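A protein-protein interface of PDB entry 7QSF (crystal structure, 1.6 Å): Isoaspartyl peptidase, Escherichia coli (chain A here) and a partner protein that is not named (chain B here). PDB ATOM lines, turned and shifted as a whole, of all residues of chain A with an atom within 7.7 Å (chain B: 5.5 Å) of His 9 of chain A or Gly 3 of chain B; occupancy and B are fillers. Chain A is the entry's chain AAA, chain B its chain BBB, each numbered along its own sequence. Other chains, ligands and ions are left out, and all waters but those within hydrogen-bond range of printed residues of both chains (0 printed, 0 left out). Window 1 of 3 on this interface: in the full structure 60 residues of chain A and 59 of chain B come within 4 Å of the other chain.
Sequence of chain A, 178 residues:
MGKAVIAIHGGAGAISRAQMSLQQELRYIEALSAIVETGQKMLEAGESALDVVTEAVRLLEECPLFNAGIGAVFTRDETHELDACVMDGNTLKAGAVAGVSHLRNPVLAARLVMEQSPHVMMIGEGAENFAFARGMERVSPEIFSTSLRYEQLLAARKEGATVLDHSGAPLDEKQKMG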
ATOM      1  N   ILE A   6      28.315 -12.999   0.000  1.00  0.00           N
ATOM      2  CA  ILE A   6      28.398 -11.762   0.825  1.00  0.00           C
ATOM      3  C   ILE A   6      28.220 -12.146   2.287  1.00  0.00           C
ATOM      4  O   ILE A   6      27.381 -13.010   2.560  1.00  0.00           O
ATOM      5  CB  ILE A   6      27.331 -10.743   0.396  1.00  0.00           C
ATOM      6  CG1 ILE A   6      27.416  -9.480   1.250  1.00  0.00           C
ATOM      7  CG2 ILE A   6      25.938 -11.359   0.401  1.00  0.00           C
ATOM      8  CD1 ILE A   6      26.534  -8.337   0.846  1.00  0.00           C
ATOM      9  N   ALA A   7      29.018 -11.549   3.169  1.00  0.00           N
ATOM     10  CA  ALA A   7      28.758 -11.497   4.630  1.00  0.00           C
ATOM     11  C   ALA A   7      28.683 -10.038   5.085  1.00  0.00           C
ATOM     12  O   ALA A   7      29.418  -9.181   4.531  1.00  0.00           O
ATOM     13  CB  ALA A   7      29.805 -12.248   5.428  1.00  0.00           C
ATOM     14  N   ILE A   8      27.836  -9.760   6.080  1.00  0.00           N
ATOM     15  CA  ILE A   8      27.753  -8.404   6.701  1.00  0.00           C
ATOM     16  C   ILE A   8      27.754  -8.566   8.235  1.00  0.00           C
ATOM     17  O   ILE A   8      27.363  -9.639   8.722  1.00  0.00           O
ATOM     18  CB  ILE A   8      26.496  -7.632   6.244  1.00  0.00           C
ATOM     19  CG1 ILE A   8      25.201  -8.334   6.702  1.00  0.00           C
ATOM     20  CG2 ILE A   8      26.518  -7.322   4.734  1.00  0.00           C
ATOM     21  CD1 ILE A   8      23.926  -7.577   6.387  1.00  0.00           C
ATOM     22  N   HIS A   9      28.079  -7.501   8.972  1.00  0.00           N
ATOM     23  CA  HIS A   9      27.922  -7.424  10.449  1.00  0.00           C
ATOM     24  C   HIS A   9      27.446  -6.032  10.859  1.00  0.00           C
ATOM     25  O   HIS A   9      27.636  -5.099  10.060  1.00  0.00           O
ATOM     26  CB  HIS A   9      29.225  -7.821  11.157  1.00  0.00           C
ATOM     27  CG  HIS A   9      30.255  -6.742  11.185  1.00  0.00           C
ATOM     28  ND1 HIS A   9      30.242  -5.747  12.132  1.00  0.00           N
ATOM     29  CD2 HIS A   9      31.322  -6.477  10.392  1.00  0.00           C
ATOM     30  CE1 HIS A   9      31.232  -4.905  11.912  1.00  0.00           C
ATOM     31  NE2 HIS A   9      31.936  -5.359  10.888  1.00  0.00           N
ATOM     32  N   GLY A  10      26.775  -5.948  12.018  1.00  0.00           N
ATOM     33  CA  GLY A  10      26.302  -4.693  12.621  1.00  0.00           C
ATOM     34  C   GLY A  10      26.786  -4.576  14.042  1.00  0.00           C
ATOM     35  O   GLY A  10      26.113  -3.879  14.808  1.00  0.00           O
ATOM     36  N   GLY A  11      27.951  -5.184  14.327  1.00  0.00           N
ATOM     37  CA  GLY A  11      28.699  -5.046  15.585  1.00  0.00           C
ATOM     38  C   GLY A  11      28.606  -6.231  16.542  1.00  0.00           C
ATOM     39  O   GLY A  11      27.587  -6.940  16.564  1.00  0.00           O
ATOM     40  N   ALA A  12      29.660  -6.404  17.344  1.00  0.00           N
ATOM     41  CA  ALA A  12      29.834  -7.467  18.359  1.00  0.00           C
ATOM     42  C   ALA A  12      29.776  -6.818  19.732  1.00  0.00           C
ATOM     43  O   ALA A  12      30.277  -5.692  19.871  1.00  0.00           O
ATOM     44  CB  ALA A  12      31.159  -8.162  18.173  1.00  0.00           C
ATOM     45  N   LEU A  32      19.050  -7.004   8.851  1.00  0.00           N
ATOM     46  CA  LEU A  32      20.198  -7.764   8.318  1.00  0.00           C
ATOM     47  C   LEU A  32      19.749  -8.520   7.070  1.00  0.00           C
ATOM     48  O   LEU A  32      20.485  -8.522   6.050  1.00  0.00           O
ATOM     49  CB  LEU A  32      20.702  -8.728   9.389  1.00  0.00           C
ATOM     50  CG  LEU A  32      21.298  -8.068  10.630  1.00  0.00           C
ATOM     51  CD1 LEU A  32      21.290  -9.079  11.772  1.00  0.00           C
ATOM     52  CD2 LEU A  32      22.695  -7.556  10.381  1.00  0.00           C
ATOM     53  N   ILE A  35      19.422  -6.303   3.834  1.00  0.00           N
ATOM     54  CA  ILE A  35      20.730  -5.812   3.311  1.00  0.00           C
ATOM     55  C   ILE A  35      21.465  -6.985   2.616  1.00  0.00           C
ATOM     56  O   ILE A  35      22.006  -6.777   1.513  1.00  0.00           O
ATOM     57  CB  ILE A  35      21.508  -5.085   4.432  1.00  0.00           C
ATOM     58  CG1 ILE A  35      20.728  -3.856   4.934  1.00  0.00           C
ATOM     59  CG2 ILE A  35      22.920  -4.707   4.040  1.00  0.00           C
ATOM     60  CD1 ILE A  35      21.273  -3.226   6.187  1.00  0.00           C
ATOM     61  N   VAL A  53      30.039  -4.289  -1.568  1.00  0.00           N
ATOM     62  CA  VAL A  53      30.378  -3.990  -0.158  1.00  0.00           C
ATOM     63  C   VAL A  53      30.111  -2.507   0.110  1.00  0.00           C
ATOM     64  O   VAL A  53      29.742  -2.165   1.240  1.00  0.00           O
ATOM     65  CB  VAL A  53      31.805  -4.422   0.246  1.00  0.00           C
ATOM     66  CG1 VAL A  53      31.979  -5.913   0.103  1.00  0.00           C
ATOM     67  CG2 VAL A  53      32.921  -3.666  -0.470  1.00  0.00           C
ATOM     68  N   ALA A  56      26.259  -2.274   0.599  1.00  0.00           N
ATOM     69  CA  ALA A  56      25.854  -2.939   1.854  1.00  0.00           C
ATOM     70  C   ALA A  56      26.195  -2.039   3.048  1.00  0.00           C
ATOM     71  O   ALA A  56      25.347  -1.876   3.972  1.00  0.00           O
ATOM     72  CB  ALA A  56      26.470  -4.314   1.971  1.00  0.00           C
ATOM     73  N   VAL A  57      27.405  -1.469   3.078  1.00  0.00           N
ATOM     74  CA  VAL A  57      27.746  -0.572   4.210  1.00  0.00           C
ATOM     75  C   VAL A  57      26.944   0.730   4.101  1.00  0.00           C
ATOM     76  O   VAL A  57      26.568   1.275   5.181  1.00  0.00           O
ATOM     77  CB  VAL A  57      29.271  -0.377   4.364  1.00  0.00           C
ATOM     78  CG1 VAL A  57      29.627   0.633   5.452  1.00  0.00           C
ATOM     79  CG2 VAL A  57      29.976  -1.710   4.627  1.00  0.00           C
ATOM     80  N   LEU A  60      23.769  -0.196   5.908  1.00  0.00           N
ATOM     81  CA  LEU A  60      24.002  -0.369   7.367  1.00  0.00           C
ATOM     82  C   LEU A  60      24.142   1.018   8.026  1.00  0.00           C
ATOM     83  O   LEU A  60      23.667   1.210   9.155  1.00  0.00           O
ATOM     84  CB  LEU A  60      25.231  -1.252   7.557  1.00  0.00           C
ATOM     85  CG  LEU A  60      25.040  -2.737   7.197  1.00  0.00           C
ATOM     86  CD1 LEU A  60      26.379  -3.425   6.943  1.00  0.00           C
ATOM     87  CD2 LEU A  60      24.247  -3.497   8.255  1.00  0.00           C
ATOM     88  N   PHE A  66      22.054   0.293  13.808  1.00  0.00           N
ATOM     89  CA  PHE A  66      23.501  -0.034  13.768  1.00  0.00           C
ATOM     90  C   PHE A  66      24.349   1.239  13.901  1.00  0.00           C
ATOM     91  O   PHE A  66      24.010   2.276  13.320  1.00  0.00           O
ATOM     92  CB  PHE A  66      23.813  -0.895  12.537  1.00  0.00           C
ATOM     93  CG  PHE A  66      22.999  -2.160  12.461  1.00  0.00           C
ATOM     94  CD1 PHE A  66      23.030  -3.091  13.505  1.00  0.00           C
ATOM     95  CD2 PHE A  66      22.179  -2.417  11.379  1.00  0.00           C
ATOM     96  CE1 PHE A  66      22.256  -4.244  13.435  1.00  0.00           C
ATOM     97  CE2 PHE A  66      21.424  -3.582  11.300  1.00  0.00           C
ATOM     98  CZ  PHE A  66      21.452  -4.481  12.346  1.00  0.00           C
ATOM     99  N   ALA A  68      26.813   3.224  12.892  1.00  0.00           N
ATOM    100  CA  ALA A  68      27.524   3.834  11.751  1.00  0.00           C
ATOM    101  C   ALA A  68      26.509   4.794  11.137  1.00  0.00           C
ATOM    102  O   ALA A  68      25.322   4.424  11.111  1.00  0.00           O
ATOM    103  CB  ALA A  68      27.997   2.789  10.721  1.00  0.00           C
ATOM    104  N   CYS A  85      36.423   2.867   6.023  1.00  0.00           N
ATOM    105  CA  CYS A  85      37.449   2.367   5.065  1.00  0.00           C
ATOM    106  C   CYS A  85      36.824   1.379   4.088  1.00  0.00           C
ATOM    107  O   CYS A  85      35.890   0.642   4.506  1.00  0.00           O
ATOM    108  CB  CYS A  85      38.571   1.658   5.800  1.00  0.00           C
ATOM    109  SG  CYS A  85      40.002   1.137   4.801  1.00  0.00           S
ATOM    110  N   THR B   1      30.309  -0.042  15.106  1.00  0.00           N
ATOM    111  CA  THR B   1      30.868  -0.514  13.820  1.00  0.00           C
ATOM    112  C   THR B   1      29.897  -1.422  13.050  1.00  0.00           C
ATOM    113  O   THR B   1      29.114  -2.234  13.702  1.00  0.00           O
ATOM    114  CB  THR B   1      32.200  -1.212  14.075  1.00  0.00           C
ATOM    115  OG1 THR B   1      32.837  -0.269  14.937  1.00  0.00           O
ATOM    116  CG2 THR B   1      32.983  -1.484  12.818  1.00  0.00           C
ATOM    117  N   VAL B   2      29.921  -1.269  11.714  1.00  0.00           N
ATOM    118  CA  VAL B   2      29.232  -2.175  10.739  1.00  0.00           C
ATOM    119  C   VAL B   2      30.238  -2.581   9.646  1.00  0.00           C
ATOM    120  O   VAL B   2      31.248  -1.871   9.505  1.00  0.00           O
ATOM    121  CB  VAL B   2      28.002  -1.482  10.120  1.00  0.00           C
ATOM    122  CG1 VAL B   2      27.085  -0.912  11.186  1.00  0.00           C
ATOM    123  CG2 VAL B   2      28.413  -0.382   9.120  1.00  0.00           C
ATOM    124  N   GLY B   3      29.991  -3.659   8.891  1.00  0.00           N
ATOM    125  CA  GLY B   3      30.899  -3.965   7.767  1.00  0.00           C
ATOM    126  C   GLY B   3      30.357  -4.990   6.801  1.00  0.00           C
ATOM    127  O   GLY B   3      29.304  -5.552   7.035  1.00  0.00           O
ATOM    128  N   ALA B   4      31.058  -5.168   5.681  1.00  0.00           N
ATOM    129  CA  ALA B   4      30.665  -6.125   4.625  1.00  0.00           C
ATOM    130  C   ALA B   4      31.921  -6.630   3.920  1.00  0.00           C
ATOM    131  O   ALA B   4      32.855  -5.816   3.692  1.00  0.00           O
ATOM    132  CB  ALA B   4      29.688  -5.502   3.667  1.00  0.00           C
ATOM    133  N   VAL B   5      31.872  -7.896   3.514  1.00  0.00           N
ATOM    134  CA  VAL B   5      32.898  -8.564   2.648  1.00  0.00           C
ATOM    135  C   VAL B   5      32.187  -9.307   1.498  1.00  0.00           C
ATOM    136  O   VAL B   5      31.044  -9.752   1.684  1.00  0.00           O
ATOM    137  CB  VAL B   5      33.814  -9.501   3.486  1.00  0.00           C
ATOM    138  CG1 VAL B   5      34.678  -8.683   4.460  1.00  0.00           C
ATOM    139  CG2 VAL B   5      33.019 -10.590   4.216  1.00  0.00           C
ATOM    140  N   ALA B  16      34.652  -3.585   3.421  1.00  0.00           N
ATOM    141  CA  ALA B  16      34.370  -2.203   3.889  1.00  0.00           C
ATOM    142  C   ALA B  16      33.905  -2.226   5.328  1.00  0.00           C
ATOM    143  O   ALA B  16      33.219  -3.213   5.735  1.00  0.00           O
ATOM    144  CB  ALA B  16      33.315  -1.537   3.021  1.00  0.00           C
ATOM    145  N   THR B  17      34.191  -1.110   6.037  1.00  0.00           N
ATOM    146  CA  THR B  17      33.906  -0.949   7.477  1.00  0.00           C
ATOM    147  C   THR B  17      33.545   0.507   7.757  1.00  0.00           C
ATOM    148  O   THR B  17      34.185   1.345   7.129  1.00  0.00           O
ATOM    149  CB  THR B  17      35.121  -1.345   8.332  1.00  0.00           C
ATOM    150  OG1 THR B  17      35.610  -2.616   7.896  1.00  0.00           O
ATOM    151  CG2 THR B  17      34.758  -1.368   9.801  1.00  0.00           C
ATOM    152  N   SER B  18      32.584   0.764   8.651  1.00  0.00           N
ATOM    153  CA  SER B  18      32.085   2.117   9.013  1.00  0.00           C
ATOM    154  C   SER B  18      31.674   2.121  10.489  1.00  0.00           C
ATOM    155  O   SER B  18      31.088   1.114  10.904  1.00  0.00           O
ATOM    156  CB  SER B  18      30.942   2.546   8.128  1.00  0.00           C
ATOM    157  OG  SER B  18      30.599   3.914   8.411  1.00  0.00           O
ATOM    158  N   SER B  50      36.441  -7.753   7.515  1.00  0.00           N
ATOM    159  CA  SER B  50      35.913  -6.543   8.213  1.00  0.00           C
ATOM    160  C   SER B  50      35.722  -6.879   9.697  1.00  0.00           C
ATOM    161  O   SER B  50      35.116  -7.905  10.014  1.00  0.00           O
ATOM    162  CB  SER B  50      34.624  -5.993   7.608  1.00  0.00           C
ATOM    163  OG  SER B  50      34.092  -4.911   8.383  1.00  0.00           O
ATOM    164  N   CYS B  51      36.254  -6.043  10.568  1.00  0.00           N
ATOM    165  CA  CYS B  51      36.336  -6.289  12.034  1.00  0.00           C
ATOM    166  C   CYS B  51      35.389  -5.406  12.860  1.00  0.00           C
ATOM    167  O   CYS B  51      35.000  -4.267  12.460  1.00  0.00           O
ATOM    168  CB  CYS B  51      37.750  -6.034  12.538  1.00  0.00           C
ATOM    169  SG  CYS B  51      38.953  -7.200  11.877  1.00  0.00           S
ATOM    170  N   THR B  52      35.038  -5.933  14.024  1.00  0.00           N
ATOM    171  CA  THR B  52      34.338  -5.087  15.073  1.00  0.00           C
ATOM    172  C   THR B  52      34.823  -5.433  16.477  1.00  0.00           C
ATOM    173  O   THR B  52      34.815  -6.613  16.814  1.00  0.00           O
ATOM    174  CB  THR B  52      32.815  -5.260  15.013  1.00  0.00           C
ATOM    175  OG1 THR B  52      32.160  -4.664  16.124  1.00  0.00           O
ATOM    176  CG2 THR B  52      32.403  -6.712  14.931  1.00  0.00           C
ATOM    177  N   ILE B 100      34.214 -10.721  10.162  1.00  0.00           N
ATOM    178  CA  ILE B 100      33.637 -11.487   9.026  1.00  0.00           C
ATOM    179  C   ILE B 100      34.709 -11.605   7.943  1.00  0.00           C
ATOM    180  O   ILE B 100      35.452 -10.604   7.674  1.00  0.00           O
ATOM    181  CB  ILE B 100      32.340 -10.829   8.520  1.00  0.00           C
ATOM    182  CG1 ILE B 100      32.591  -9.430   7.949  1.00  0.00           C
ATOM    183  CG2 ILE B 100      31.287 -10.833   9.642  1.00  0.00           C
ATOM    184  CD1 ILE B 100      31.362  -8.715   7.409  1.00  0.00           C
ATOM    185  N   MET B 117      27.006 -11.067  18.074  1.00  0.00           N
ATOM    186  CA  MET B 117      27.468 -10.213  16.943  1.00  0.00           C
ATOM    187  C   MET B 117      26.342 -10.236  15.899  1.00  0.00           C
ATOM    188  O   MET B 117      25.979 -11.313  15.444  1.00  0.00           O
ATOM    189  CB  MET B 117      28.797 -10.714  16.344  1.00  0.00           C
ATOM    190  CG  MET B 117      29.235  -9.911  15.166  1.00  0.00           C
ATOM    191  SD  MET B 117      30.929 -10.201  14.547  1.00  0.00           S
ATOM    192  CE  MET B 117      30.756 -11.709  13.592  1.00  0.00           C
ATOM    193  N   TYR B 118      25.727  -9.083  15.633  1.00  0.00           N
ATOM    194  CA  TYR B 118      24.685  -8.920  14.593  1.00  0.00           C
ATOM    195  C   TYR B 118      25.320  -9.277  13.262  1.00  0.00           C
ATOM    196  O   TYR B 118      26.343  -8.644  12.958  1.00  0.00           O
ATOM    197  CB  TYR B 118      24.138  -7.500  14.587  1.00  0.00           C
ATOM    198  CG  TYR B 118      23.368  -7.131  15.823  1.00  0.00           C
ATOM    199  CD1 TYR B 118      22.130  -7.699  16.086  1.00  0.00           C
ATOM    200  CD2 TYR B 118      23.869  -6.226  16.735  1.00  0.00           C
ATOM    201  CE1 TYR B 118      21.399  -7.359  17.208  1.00  0.00           C
ATOM    202  CE2 TYR B 118      23.126  -5.844  17.832  1.00  0.00           C
ATOM    203  CZ  TYR B 118      21.903  -6.430  18.085  1.00  0.00           C
ATOM    204  OH  TYR B 118      21.203  -6.081  19.204  1.00  0.00           O
ATOM    205  N   ARG B 119      24.794 -10.281  12.556  1.00  0.00           N
ATOM    206  CA  ARG B 119      25.515 -10.809  11.380  1.00  0.00           C
ATOM    207  C   ARG B 119      24.572 -11.550  10.442  1.00  0.00           C
ATOM    208  O   ARG B 119      23.507 -12.067  10.882  1.00  0.00           O
ATOM    209  CB  ARG B 119      26.639 -11.751  11.808  1.00  0.00           C
ATOM    210  CG  ARG B 119      26.127 -13.097  12.302  1.00  0.00           C
ATOM    211  CD  ARG B 119      27.167 -13.745  13.178  1.00  0.00           C
ATOM    212  NE  ARG B 119      26.761 -15.049  13.693  1.00  0.00           N
ATOM    213  CZ  ARG B 119      26.177 -15.302  14.869  1.00  0.00           C
ATOM    214  NH1 ARG B 119      25.835 -14.335  15.707  1.00  0.00           N
ATOM    215  NH2 ARG B 119      25.887 -16.554  15.180  1.00  0.00           N
ATOM    216  N   ALA B 120      24.949 -11.592   9.154  1.00  0.00           N
ATOM    217  CA  ALA B 120      24.205 -12.339   8.124  1.00  0.00           C
ATOM    218  C   ALA B 120      25.123 -12.660   6.933  1.00  0.00           C
ATOM    219  O   ALA B 120      26.115 -11.930   6.730  1.00  0.00           O
ATOM    220  CB  ALA B 120      22.954 -11.573   7.754  1.00  0.00           C
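The backbone carbonyl oxygen (O) of Ala 7 of chain A is in hydrogen-bond range of the backbone NH (N) of Val 5 of chain B (3.0 Å). O of Ala 120 of chain B lies within hydrogen-bond range of N of Ile 8 of chain A (2.8 Å). N of Gly 3 of chain B lies within hydrogen-bond range of O of His 9 of chain A, 3.0 Å away. A ring nitrogen (NE2) of His 9 of chain A is in hydrogen-bond range of the side-chain hydroxyl (OG) of Ser 50 of chain B (3.3 Å). N of Gly 10 of chain A is in hydrogen-bond range of O of Tyr 118 of chain B (2.9 Å). The backbone carbonyl oxygen of Thr 1 of chain B sits at hydrogen-bond distance from the backbone NH of Gly 11 of chain A. The backbone NH (N) of Tyr 118 of chain B is in hydrogen-bond range of the backbone carbonyl oxygen (O) of Gly 11 of chain A, at 3.0 Å. The backbone NH (N) of Ala 12 of chain A sits at hydrogen-bond distance from the side-chain hydroxyl (OG1) of Thr 52 of chain B (3.3 Å). The backbone carbonyl oxygen (O) of Cys 85 of chain A lies within hydrogen-bond range of the backbone NH (N) of Thr 17 of chain B, 2.9 Å away.
ND1 of His 9 of chain A lies within hydrogen-bond range of N of Gly 11 of chain A, at 3.2 Å. The backbone NH (N) of Val 2 of chain B lies within hydrogen-bond range of the backbone carbonyl oxygen (O) of Ser 18 of chain B (2.8 Å). The backbone carbonyl oxygen of Ala 4 of chain B is in hydrogen-bond range of the backbone NH of Ala 16 of chain B, 2.9 Å away. OG1 of Thr 17 of chain B is in hydrogen-bond range of OG of Ser 50 of chain B (2.8 Å). O of Ser 50 of chain B lies within hydrogen-bond range of N of Ile 100 of chain B (3.0 Å). NH1 of Arg 119 of chain B is in hydrogen-bond range of O of Met 117 of chain B, at 3.0 Å.
CA of Ala 7 of chain A touches O of Ala 120 of chain B, 3.4 Å away. Ile 100 of chain B touches Ile 8 of chain A (CD1 to CA, 3.7 Å). His 9 of chain A touches Cys 51 of chain B. Tyr 118 of chain B touches His 9 of chain A. O of Thr 1 of chain B touches C of Gly 10 of chain A (3.3 Å). CA of Met 117 of chain B touches CA of Ala 12 of chain A, at 3.9 Å. Val 57 of chain A touches Val 2 of chain B. Val 57 of chain A touches Gly 3 of chain B. Phe 66 of chain A touches Val 2 of chain B. Ser 18 of chain B touches Ala 68 of chain A.
Of chain B, only Thr 1, Val 2, Gly 3, Ser 50, Cys 51, Thr 52, Ile 100 and Tyr 118 come within 4 Å of His 9 of chain A. Of chain A, only Ile 8, His 9, Val 57 and Leu 60 come within 4 Å of Gly 3 of chain B. Of the printed residues of chain B, Ala 7 of chain A touches Ala 4 (3.3 Å), Val 5 (3.0 Å), Ile 100 (3.5 Å) and Ala 120 (3.4 Å). Of the printed residues of chain B, Ile 6 of chain A touches Val 5 (3.4 Å). Printed residues of chain A within 4 Å of Val 5 of chain B: Ile 6 (3.4 Å), Ala 7 (3.0 Å) and Val 53 (3.7 Å). Of the printed residues of chain A, Thr 17 of chain B touches Cys 85 (2.9 Å). Ile 35 of chain A touches none of the printed residues of chain B. The nearest residue of chain B that does not touch His 9 of chain A is Arg 119 of chain B (4.3 Å). The nearest residue of chain A that does not touch Gly 3 of chain B is Ala 7 of chain A (4.4 Å).
Of the 16 printed residues of chain B, 16 touch a printed residue of chain A. Among the printed residues, no Asp or Glu carboxylate lies within 4 Å of a Lys or Arg side-chain nitrogen of the other chain.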
